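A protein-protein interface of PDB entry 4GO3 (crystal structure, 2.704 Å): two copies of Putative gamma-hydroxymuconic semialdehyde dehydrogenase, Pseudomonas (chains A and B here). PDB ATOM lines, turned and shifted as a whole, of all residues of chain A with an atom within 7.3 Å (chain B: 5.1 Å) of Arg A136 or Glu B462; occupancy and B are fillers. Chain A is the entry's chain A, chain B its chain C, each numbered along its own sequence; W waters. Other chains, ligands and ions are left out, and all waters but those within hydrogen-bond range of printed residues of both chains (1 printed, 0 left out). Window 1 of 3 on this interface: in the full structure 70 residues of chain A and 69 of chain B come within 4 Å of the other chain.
Printed residues of chain B within 4 Å of Val A134: Pro B446.
Arg A136 touches just one residue of chain B: Glu B462.
Printed residues of chain B within 4 Å of Ser A472: Pro B446 (3.8 Å).
Printed residues of chain A within 4 Å of Pro B446: Val A134 (3.95 Å) and Ser A472 (3.8 Å).
Of the printed residues of chain A, Arg B457 touches Ala A470 (2.5 Å).
Printed residues of chain A within 4 Å of Glu B462: Arg A136 and His A465.
Ile B464 touches none of the printed residues of chain A.
Of the printed residues of chain A, His B465 touches His A465 (3.0 Å).
The nearest printed residue of chain B that does not touch Arg A136 is Arg B457 (6.4 Å).
The nearest residue of chain A that does not touch Glu B462 is Ala A470 (4.8 Å).
His A465 touches its own counterpart, His B465.
Of the 6 pairs that touch across the chains among the printed residues, 1 has its exchanged pair printed and touching as well.
Hydrophobic or aromatic side chains of chain A within 4 Å of the printed part of chain B: Val A134, His A465 and Ala A470.
Of the 10 printed residues of chain B, 4 touch a printed residue of chain A.
Hydrophobic or aromatic side chains of chain B within 4 Å of the printed part of chain A: Pro B446 and His B465.
Among the printed residues, Asp or Glu carboxylates within 4 Å of a Lys or Arg side-chain nitrogen of the other chain: Arg A136 with Glu B462.
CG2 of Val A134 touches CD of Pro B446, 3.95 Å away.
Ser A472 touches Pro B446.
The guanidinium group (NH2) of Arg A136 sits at hydrogen-bond distance from the backbone carbonyl oxygen (O) of His A465 (3.5 Å).
NH2 of Arg A136 lies within hydrogen-bond range of OG1 of Thr A468 (2.5 Å).
N of Val A134 sits at hydrogen-bond distance from O of Ser A122, at 2.7 Å.
OG1 of Thr A468 lies within hydrogen-bond range of O of His A465 (3.3 Å).
Water W1 lies within hydrogen-bond range of O of Pro B446 (2.7 Å), NE of Arg B457 (2.7 Å) and O of Ala A470 (3.3 Å).
OE1 of Glu B462 is in hydrogen-bond range of NE2 of His A465 (3.0 Å).
O of Ala A470 is in hydrogen-bond range of NH2 of Arg B457, 2.5 Å away.
The guanidinium group (NH1) of Arg A136 is in salt-bridge range of the side-chain carboxylate (OE2) of Glu B462.
A ring nitrogen (ND1) of His A465 sits close to a ring nitrogen (ND1) of His B465 (3.5 Å).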
ATOM      1  N   ILE A 119      12.017 -20.549  16.794  1.00  0.00           N
ATOM      2  CA  ILE A 119      10.647 -20.222  17.116  1.00  0.00           C
ATOM      3  C   ILE A 119      10.376 -20.806  18.484  1.00  0.00           C
ATOM      4  O   ILE A 119      10.270 -22.020  18.642  1.00  0.00           O
ATOM      5  CB  ILE A 119       9.694 -20.850  16.087  1.00  0.00           C
ATOM      6  CG1 ILE A 119       9.967 -20.282  14.696  1.00  0.00           C
ATOM      7  CG2 ILE A 119       8.257 -20.601  16.467  1.00  0.00           C
ATOM      8  CD1 ILE A 119       9.117 -20.896  13.581  1.00  0.00           C
ATOM      9  N   GLU A 120      10.266 -19.946  19.486  1.00  0.00           N
ATOM     10  CA  GLU A 120      10.193 -20.443  20.855  1.00  0.00           C
ATOM     11  C   GLU A 120       8.902 -20.107  21.550  1.00  0.00           C
ATOM     12  O   GLU A 120       8.316 -19.059  21.305  1.00  0.00           O
ATOM     13  CB  GLU A 120      11.371 -19.918  21.666  1.00  0.00           C
ATOM     14  CG  GLU A 120      12.686 -20.439  21.162  1.00  0.00           C
ATOM     15  CD  GLU A 120      13.854 -19.989  21.996  1.00  0.00           C
ATOM     16  OE1 GLU A 120      13.652 -19.165  22.924  1.00  0.00           O
ATOM     17  OE2 GLU A 120      14.972 -20.475  21.729  1.00  0.00           O
ATOM     18  N   GLY A 121       8.464 -21.018  22.414  1.00  0.00           N
ATOM     19  CA  GLY A 121       7.308 -20.773  23.247  1.00  0.00           C
ATOM     20  C   GLY A 121       7.781 -20.024  24.470  1.00  0.00           C
ATOM     21  O   GLY A 121       8.874 -19.465  24.493  1.00  0.00           O
ATOM     22  N   SER A 122       6.967 -20.010  25.508  1.00  0.00           N
ATOM     23  CA  SER A 122       7.343 -19.309  26.717  1.00  0.00           C
ATOM     24  C   SER A 122       6.817 -20.063  27.908  1.00  0.00           C
ATOM     25  O   SER A 122       5.932 -20.902  27.783  1.00  0.00           O
ATOM     26  CB  SER A 122       6.789 -17.883  26.691  1.00  0.00           C
ATOM     27  OG  SER A 122       5.621 -17.801  25.887  1.00  0.00           O
ATOM     28  N   VAL A 134       3.685 -22.373  27.309  1.00  0.00           N
ATOM     29  CA  VAL A 134       2.887 -22.079  26.137  1.00  0.00           C
ATOM     30  C   VAL A 134       3.692 -22.395  24.910  1.00  0.00           C
ATOM     31  O   VAL A 134       4.645 -21.705  24.606  1.00  0.00           O
ATOM     32  CB  VAL A 134       2.492 -20.615  26.098  1.00  0.00           C
ATOM     33  CG1 VAL A 134       1.652 -20.320  24.858  1.00  0.00           C
ATOM     34  CG2 VAL A 134       1.730 -20.274  27.370  1.00  0.00           C
ATOM     35  N   GLN A 135       3.332 -23.416  24.172  1.00  0.00           N
ATOM     36  CA  GLN A 135       4.027 -23.649  22.934  1.00  0.00           C
ATOM     37  C   GLN A 135       3.476 -22.783  21.829  1.00  0.00           C
ATOM     38  O   GLN A 135       2.406 -22.232  21.932  1.00  0.00           O
ATOM     39  CB  GLN A 135       3.932 -25.106  22.529  1.00  0.00           C
ATOM     40  CG  GLN A 135       4.053 -26.034  23.674  1.00  0.00           C
ATOM     41  CD  GLN A 135       4.619 -27.344  23.277  1.00  0.00           C
ATOM     42  OE1 GLN A 135       3.968 -28.363  23.396  1.00  0.00           O
ATOM     43  NE2 GLN A 135       5.845 -27.335  22.804  1.00  0.00           N
ATOM     44  N   ARG A 136       4.249 -22.671  20.766  1.00  0.00           N
ATOM     45  CA  ARG A 136       3.829 -22.027  19.543  1.00  0.00           C
ATOM     46  C   ARG A 136       3.715 -23.128  18.541  1.00  0.00           C
ATOM     47  O   ARG A 136       4.707 -23.670  18.119  1.00  0.00           O
ATOM     48  CB  ARG A 136       4.898 -21.080  19.049  1.00  0.00           C
ATOM     49  CG  ARG A 136       5.422 -20.167  20.052  1.00  0.00           C
ATOM     50  CD  ARG A 136       4.474 -19.038  20.254  1.00  0.00           C
ATOM     51  NE  ARG A 136       3.792 -18.630  19.039  1.00  0.00           N
ATOM     52  CZ  ARG A 136       2.765 -17.794  19.018  1.00  0.00           C
ATOM     53  NH1 ARG A 136       2.306 -17.289  20.146  1.00  0.00           N
ATOM     54  NH2 ARG A 136       2.197 -17.458  17.881  1.00  0.00           N
ATOM     55  N   LYS A 137       2.509 -23.484  18.163  1.00  0.00           N
ATOM     56  CA  LYS A 137       2.375 -24.547  17.216  1.00  0.00           C
ATOM     57  C   LYS A 137       1.964 -23.972  15.893  1.00  0.00           C
ATOM     58  O   LYS A 137       1.485 -22.857  15.817  1.00  0.00           O
ATOM     59  CB  LYS A 137       1.372 -25.566  17.721  1.00  0.00           C
ATOM     60  CG  LYS A 137       1.828 -26.288  18.964  1.00  0.00           C
ATOM     61  CD  LYS A 137       2.560 -27.571  18.635  1.00  0.00           C
ATOM     62  CE  LYS A 137       3.738 -27.830  19.553  1.00  0.00           C
ATOM     63  NZ  LYS A 137       5.063 -27.382  19.027  1.00  0.00           N
ATOM     64  N   PRO A 138       2.180 -24.737  14.841  1.00  0.00           N
ATOM     65  CA  PRO A 138       1.732 -24.342  13.516  1.00  0.00           C
ATOM     66  C   PRO A 138       0.231 -24.361  13.499  1.00  0.00           C
ATOM     67  O   PRO A 138      -0.350 -25.189  14.176  1.00  0.00           O
ATOM     68  CB  PRO A 138       2.240 -25.465  12.643  1.00  0.00           C
ATOM     69  CG  PRO A 138       3.290 -26.100  13.401  1.00  0.00           C
ATOM     70  CD  PRO A 138       2.959 -25.978  14.803  1.00  0.00           C
ATOM     71  N   ILE A 139      -0.377 -23.467  12.740  1.00  0.00           N
ATOM     72  CA  ILE A 139      -1.804 -23.443  12.557  1.00  0.00           C
ATOM     73  C   ILE A 139      -2.284 -24.743  11.940  1.00  0.00           C
ATOM     74  O   ILE A 139      -3.237 -25.356  12.401  1.00  0.00           O
ATOM     75  CB  ILE A 139      -2.182 -22.321  11.625  1.00  0.00           C
ATOM     76  CG1 ILE A 139      -1.863 -20.993  12.275  1.00  0.00           C
ATOM     77  CG2 ILE A 139      -3.636 -22.389  11.302  1.00  0.00           C
ATOM     78  CD1 ILE A 139      -1.516 -19.944  11.318  1.00  0.00           C
ATOM     79  N   ALA A 165       7.589 -22.557  10.466  1.00  0.00           N
ATOM     80  CA  ALA A 165       6.745 -22.820  11.607  1.00  0.00           C
ATOM     81  C   ALA A 165       6.071 -24.178  11.498  1.00  0.00           C
ATOM     82  O   ALA A 165       5.496 -24.656  12.441  1.00  0.00           O
ATOM     83  CB  ALA A 165       5.738 -21.727  11.768  1.00  0.00           C
ATOM     84  N   ARG A 243      -7.656 -17.709  10.211  1.00  0.00           N
ATOM     85  CA  ARG A 243      -6.987 -16.439  10.400  1.00  0.00           C
ATOM     86  C   ARG A 243      -6.638 -15.843   9.055  1.00  0.00           C
ATOM     87  O   ARG A 243      -6.546 -16.538   8.071  1.00  0.00           O
ATOM     88  CB  ARG A 243      -5.757 -16.584  11.284  1.00  0.00           C
ATOM     89  CG  ARG A 243      -5.681 -17.903  11.991  1.00  0.00           C
ATOM     90  CD  ARG A 243      -5.076 -17.764  13.343  1.00  0.00           C
ATOM     91  NE  ARG A 243      -3.884 -16.933  13.358  1.00  0.00           N
ATOM     92  CZ  ARG A 243      -2.812 -17.191  14.096  1.00  0.00           C
ATOM     93  NH1 ARG A 243      -2.779 -18.263  14.860  1.00  0.00           N
ATOM     94  NH2 ARG A 243      -1.774 -16.382  14.072  1.00  0.00           N
ATOM     95  N   ILE A 464       6.515 -15.244  11.655  1.00  0.00           N
ATOM     96  CA  ILE A 464       6.391 -16.499  12.383  1.00  0.00           C
ATOM     97  C   ILE A 464       5.221 -16.458  13.365  1.00  0.00           C
ATOM     98  O   ILE A 464       4.464 -17.415  13.497  1.00  0.00           O
ATOM     99  CB  ILE A 464       7.683 -16.826  13.167  1.00  0.00           C
ATOM    100  CG1 ILE A 464       8.769 -17.285  12.204  1.00  0.00           C
ATOM    101  CG2 ILE A 464       7.407 -17.905  14.208  1.00  0.00           C
ATOM    102  CD1 ILE A 464       8.324 -18.415  11.334  1.00  0.00           C
ATOM    103  N   HIS A 465       5.087 -15.346  14.075  1.00  0.00           N
ATOM    104  CA  HIS A 465       3.965 -15.200  14.981  1.00  0.00           C
ATOM    105  C   HIS A 465       2.652 -15.390  14.236  1.00  0.00           C
ATOM    106  O   HIS A 465       1.743 -16.010  14.735  1.00  0.00           O
ATOM    107  CB  HIS A 465       3.979 -13.835  15.662  1.00  0.00           C
ATOM    108  CG  HIS A 465       2.850 -13.637  16.616  1.00  0.00           C
ATOM    109  ND1 HIS A 465       1.622 -13.155  16.222  1.00  0.00           N
ATOM    110  CD2 HIS A 465       2.754 -13.881  17.944  1.00  0.00           C
ATOM    111  CE1 HIS A 465       0.820 -13.095  17.271  1.00  0.00           C
ATOM    112  NE2 HIS A 465       1.482 -13.530  18.330  1.00  0.00           N
ATOM    113  N   ASP A 466       2.572 -14.859  13.028  1.00  0.00           N
ATOM    114  CA  ASP A 466       1.343 -14.925  12.242  1.00  0.00           C
ATOM    115  C   ASP A 466       1.044 -16.307  11.712  1.00  0.00           C
ATOM    116  O   ASP A 466      -0.093 -16.591  11.372  1.00  0.00           O
ATOM    117  CB  ASP A 466       1.373 -13.928  11.075  1.00  0.00           C
ATOM    118  CG  ASP A 466       1.191 -12.501  11.537  1.00  0.00           C
ATOM    119  OD1 ASP A 466       0.973 -12.285  12.759  1.00  0.00           O
ATOM    120  OD2 ASP A 466       1.274 -11.599  10.680  1.00  0.00           O
ATOM    121  N   TYR A 467       1.997 -17.210  11.794  1.00  0.00           N
ATOM    122  CA  TYR A 467       1.815 -18.555  11.329  1.00  0.00           C
ATOM    123  C   TYR A 467       1.897 -19.569  12.398  1.00  0.00           C
ATOM    124  O   TYR A 467       2.132 -20.691  12.119  1.00  0.00           O
ATOM    125  CB  TYR A 467       2.835 -18.908  10.255  1.00  0.00           C
ATOM    126  CG  TYR A 467       2.523 -18.281   8.946  1.00  0.00           C
ATOM    127  CD1 TYR A 467       3.220 -17.208   8.500  1.00  0.00           C
ATOM    128  CD2 TYR A 467       1.505 -18.741   8.174  1.00  0.00           C
ATOM    129  CE1 TYR A 467       2.922 -16.638   7.345  1.00  0.00           C
ATOM    130  CE2 TYR A 467       1.208 -18.159   7.019  1.00  0.00           C
ATOM    131  CZ  TYR A 467       1.910 -17.114   6.611  1.00  0.00           C
ATOM    132  OH  TYR A 467       1.592 -16.551   5.440  1.00  0.00           O
ATOM    133  N   THR A 468       1.741 -19.160  13.636  1.00  0.00           N
ATOM    134  CA  THR A 468       1.707 -20.113  14.723  1.00  0.00           C
ATOM    135  C   THR A 468       0.514 -19.806  15.596  1.00  0.00           C
ATOM    136  O   THR A 468      -0.151 -18.811  15.407  1.00  0.00           O
ATOM    137  CB  THR A 468       2.973 -20.076  15.566  1.00  0.00           C
ATOM    138  OG1 THR A 468       3.219 -18.744  15.981  1.00  0.00           O
ATOM    139  CG2 THR A 468       4.150 -20.561  14.780  1.00  0.00           C
ATOM    140  N   GLU A 469       0.233 -20.684  16.541  1.00  0.00           N
ATOM    141  CA  GLU A 469      -0.788 -20.412  17.519  1.00  0.00           C
ATOM    142  C   GLU A 469      -0.199 -20.623  18.873  1.00  0.00           C
ATOM    143  O   GLU A 469       0.669 -21.440  19.038  1.00  0.00           O
ATOM    144  CB  GLU A 469      -1.963 -21.358  17.353  1.00  0.00           C
ATOM    145  CG  GLU A 469      -1.797 -22.333  16.246  1.00  0.00           C
ATOM    146  CD  GLU A 469      -2.516 -23.627  16.499  1.00  0.00           C
ATOM    147  OE1 GLU A 469      -1.928 -24.503  17.152  1.00  0.00           O
ATOM    148  OE2 GLU A 469      -3.660 -23.779  16.028  1.00  0.00           O
ATOM    149  N   ALA A 470      -0.693 -19.877  19.845  1.00  0.00           N
ATOM    150  CA  ALA A 470      -0.398 -20.112  21.227  1.00  0.00           C
ATOM    151  C   ALA A 470      -1.145 -21.342  21.735  1.00  0.00           C
ATOM    152  O   ALA A 470      -2.342 -21.393  21.710  1.00  0.00           O
ATOM    153  CB  ALA A 470      -0.786 -18.936  21.989  1.00  0.00           C
ATOM    154  N   ARG A 471      -0.401 -22.328  22.208  1.00  0.00           N
ATOM    155  CA  ARG A 471      -0.981 -23.477  22.871  1.00  0.00           C
ATOM    156  C   ARG A 471      -0.584 -23.510  24.354  1.00  0.00           C
ATOM    157  O   ARG A 471       0.464 -24.012  24.702  1.00  0.00           O
ATOM    158  CB  ARG A 471      -0.544 -24.752  22.167  1.00  0.00           C
ATOM    159  CG  ARG A 471      -1.052 -24.898  20.739  1.00  0.00           C
ATOM    160  CD  ARG A 471      -2.404 -25.586  20.681  1.00  0.00           C
ATOM    161  NE  ARG A 471      -2.461 -26.651  19.689  1.00  0.00           N
ATOM    162  CZ  ARG A 471      -2.901 -27.878  19.943  1.00  0.00           C
ATOM    163  NH1 ARG A 471      -3.319 -28.199  21.154  1.00  0.00           N
ATOM    164  NH2 ARG A 471      -2.925 -28.790  18.984  1.00  0.00           N
ATOM    165  N   SER A 472      -1.434 -22.970  25.223  1.00  0.00           N
ATOM    166  CA  SER A 472      -1.106 -22.877  26.650  1.00  0.00           C
ATOM    167  C   SER A 472      -1.387 -24.172  27.401  1.00  0.00           C
ATOM    168  O   SER A 472      -2.508 -24.686  27.394  1.00  0.00           O
ATOM    169  CB  SER A 472      -1.870 -21.732  27.304  1.00  0.00           C
ATOM    170  OG  SER A 472      -1.676 -21.735  28.702  1.00  0.00           O
ATOM    171  N   PRO B 446      -1.603 -16.561  27.905  1.00  0.00           N
ATOM    172  CA  PRO B 446      -2.416 -16.382  26.709  1.00  0.00           C
ATOM    173  C   PRO B 446      -3.669 -17.229  26.694  1.00  0.00           C
ATOM    174  O   PRO B 446      -3.618 -18.441  26.653  1.00  0.00           O
ATOM    175  CB  PRO B 446      -1.477 -16.825  25.608  1.00  0.00           C
ATOM    176  CG  PRO B 446      -0.183 -16.493  26.111  1.00  0.00           C
ATOM    177  CD  PRO B 446      -0.210 -16.836  27.546  1.00  0.00           C
ATOM    178  N   ARG B 457      -5.482 -13.711  21.254  1.00  0.00           N
ATOM    179  CA  ARG B 457      -5.262 -14.114  22.612  1.00  0.00           C
ATOM    180  C   ARG B 457      -5.514 -12.964  23.541  1.00  0.00           C
ATOM    181  O   ARG B 457      -5.253 -11.834  23.213  1.00  0.00           O
ATOM    182  CB  ARG B 457      -3.833 -14.623  22.778  1.00  0.00           C
ATOM    183  CG  ARG B 457      -3.583 -15.967  22.147  1.00  0.00           C
ATOM    184  CD  ARG B 457      -4.370 -17.013  22.846  1.00  0.00           C
ATOM    185  NE  ARG B 457      -4.069 -18.334  22.360  1.00  0.00           N
ATOM    186  CZ  ARG B 457      -4.639 -18.866  21.298  1.00  0.00           C
ATOM    187  NH1 ARG B 457      -5.528 -18.180  20.631  1.00  0.00           N
ATOM    188  NH2 ARG B 457      -4.314 -20.081  20.900  1.00  0.00           N
ATOM    189  N   MET B 459      -4.678 -11.795  27.497  1.00  0.00           N
ATOM    190  CA  MET B 459      -3.641 -12.062  28.477  1.00  0.00           C
ATOM    191  C   MET B 459      -2.229 -12.041  27.899  1.00  0.00           C
ATOM    192  O   MET B 459      -2.010 -12.230  26.725  1.00  0.00           O
ATOM    193  CB  MET B 459      -3.912 -13.377  29.208  1.00  0.00           C
ATOM    194  CG  MET B 459      -5.328 -13.596  29.659  1.00  0.00           C
ATOM    195  SD  MET B 459      -6.066 -12.266  30.567  1.00  0.00           S
ATOM    196  CE  MET B 459      -7.098 -13.169  31.674  1.00  0.00           C
ATOM    197  N   GLY B 460      -1.268 -11.793  28.753  1.00  0.00           N
ATOM    198  CA  GLY B 460       0.110 -11.852  28.340  1.00  0.00           C
ATOM    199  C   GLY B 460       0.472 -10.942  27.198  1.00  0.00           C
ATOM    200  O   GLY B 460      -0.363 -10.272  26.627  1.00  0.00           O
ATOM    201  N   PHE B 461       1.754 -10.944  26.870  1.00  0.00           N
ATOM    202  CA  PHE B 461       2.271 -10.143  25.787  1.00  0.00           C
ATOM    203  C   PHE B 461       1.500 -10.448  24.540  1.00  0.00           C
ATOM    204  O   PHE B 461       1.343  -9.608  23.685  1.00  0.00           O
ATOM    205  CB  PHE B 461       3.741 -10.444  25.567  1.00  0.00           C
ATOM    206  CG  PHE B 461       4.609 -10.038  26.698  1.00  0.00           C
ATOM    207  CD1 PHE B 461       5.136  -8.779  26.760  1.00  0.00           C
ATOM    208  CD2 PHE B 461       4.904 -10.919  27.701  1.00  0.00           C
ATOM    209  CE1 PHE B 461       5.920  -8.413  27.801  1.00  0.00           C
ATOM    210  CE2 PHE B 461       5.704 -10.551  28.727  1.00  0.00           C
ATOM    211  CZ  PHE B 461       6.208  -9.300  28.777  1.00  0.00           C
ATOM    212  N   GLU B 462       1.018 -11.666  24.423  1.00  0.00           N
ATOM    213  CA  GLU B 462       0.205 -11.988  23.258  1.00  0.00           C
ATOM    214  C   GLU B 462      -0.944 -11.005  23.079  1.00  0.00           C
ATOM    215  O   GLU B 462      -1.149 -10.479  21.984  1.00  0.00           O
ATOM    216  CB  GLU B 462      -0.349 -13.396  23.372  1.00  0.00           C
ATOM    217  CG  GLU B 462       0.696 -14.454  23.173  1.00  0.00           C
ATOM    218  CD  GLU B 462       1.085 -14.568  21.731  1.00  0.00           C
ATOM    219  OE1 GLU B 462       0.201 -14.342  20.887  1.00  0.00           O
ATOM    220  OE2 GLU B 462       2.261 -14.878  21.439  1.00  0.00           O
ATOM    221  N   ALA B 463      -1.693 -10.753  24.153  1.00  0.00           N
ATOM    222  CA  ALA B 463      -2.791  -9.807  24.077  1.00  0.00           C
ATOM    223  C   ALA B 463      -2.263  -8.464  23.589  1.00  0.00           C
ATOM    224  O   ALA B 463      -2.870  -7.816  22.730  1.00  0.00           O
ATOM    225  CB  ALA B 463      -3.451  -9.655  25.412  1.00  0.00           C
ATOM    226  N   ILE B 464      -1.134  -8.037  24.119  1.00  0.00           N
ATOM    227  CA  ILE B 464      -0.530  -6.793  23.701  1.00  0.00           C
ATOM    228  C   ILE B 464      -0.089  -6.832  22.244  1.00  0.00           C
ATOM    229  O   ILE B 464      -0.207  -5.854  21.537  1.00  0.00           O
ATOM    230  CB  ILE B 464       0.641  -6.473  24.579  1.00  0.00           C
ATOM    231  CG1 ILE B 464       0.139  -6.049  25.937  1.00  0.00           C
ATOM    232  CG2 ILE B 464       1.409  -5.365  23.998  1.00  0.00           C
ATOM    233  CD1 ILE B 464      -0.438  -4.710  25.931  1.00  0.00           C
ATOM    234  N   HIS B 465       0.413  -7.963  21.786  1.00  0.00           N
ATOM    235  CA  HIS B 465       0.725  -8.103  20.377  1.00  0.00           C
ATOM    236  C   HIS B 465      -0.519  -7.870  19.532  1.00  0.00           C
ATOM    237  O   HIS B 465      -0.457  -7.241  18.503  1.00  0.00           O
ATOM    238  CB  HIS B 465       1.305  -9.481  20.073  1.00  0.00           C
ATOM    239  CG  HIS B 465       1.654  -9.673  18.636  1.00  0.00           C
ATOM    240  ND1 HIS B 465       0.744 -10.121  17.705  1.00  0.00           N
ATOM    241  CD2 HIS B 465       2.808  -9.454  17.964  1.00  0.00           C
ATOM    242  CE1 HIS B 465       1.327 -10.185  16.521  1.00  0.00           C
ATOM    243  NE2 HIS B 465       2.581  -9.785  16.649  1.00  0.00           N
ATOM    244  N   ASP B 466      -1.655  -8.364  19.995  1.00  0.00           N
ATOM    245  CA  ASP B 466      -2.917  -8.260  19.276  1.00  0.00           C
ATOM    246  C   ASP B 466      -3.469  -6.856  19.206  1.00  0.00           C
ATOM    247  O   ASP B 466      -4.362  -6.569  18.438  1.00  0.00           O
ATOM    248  CB  ASP B 466      -3.940  -9.136  19.960  1.00  0.00           C
ATOM    249  CG  ASP B 466      -4.103 -10.432  19.285  1.00  0.00           C
ATOM    250  OD1 ASP B 466      -5.020 -10.528  18.474  1.00  0.00           O
ATOM    251  OD2 ASP B 466      -3.318 -11.352  19.541  1.00  0.00           O
HETATM  252  O   HOH W   1      -3.553 -19.945  24.441  1.00  0.00           O
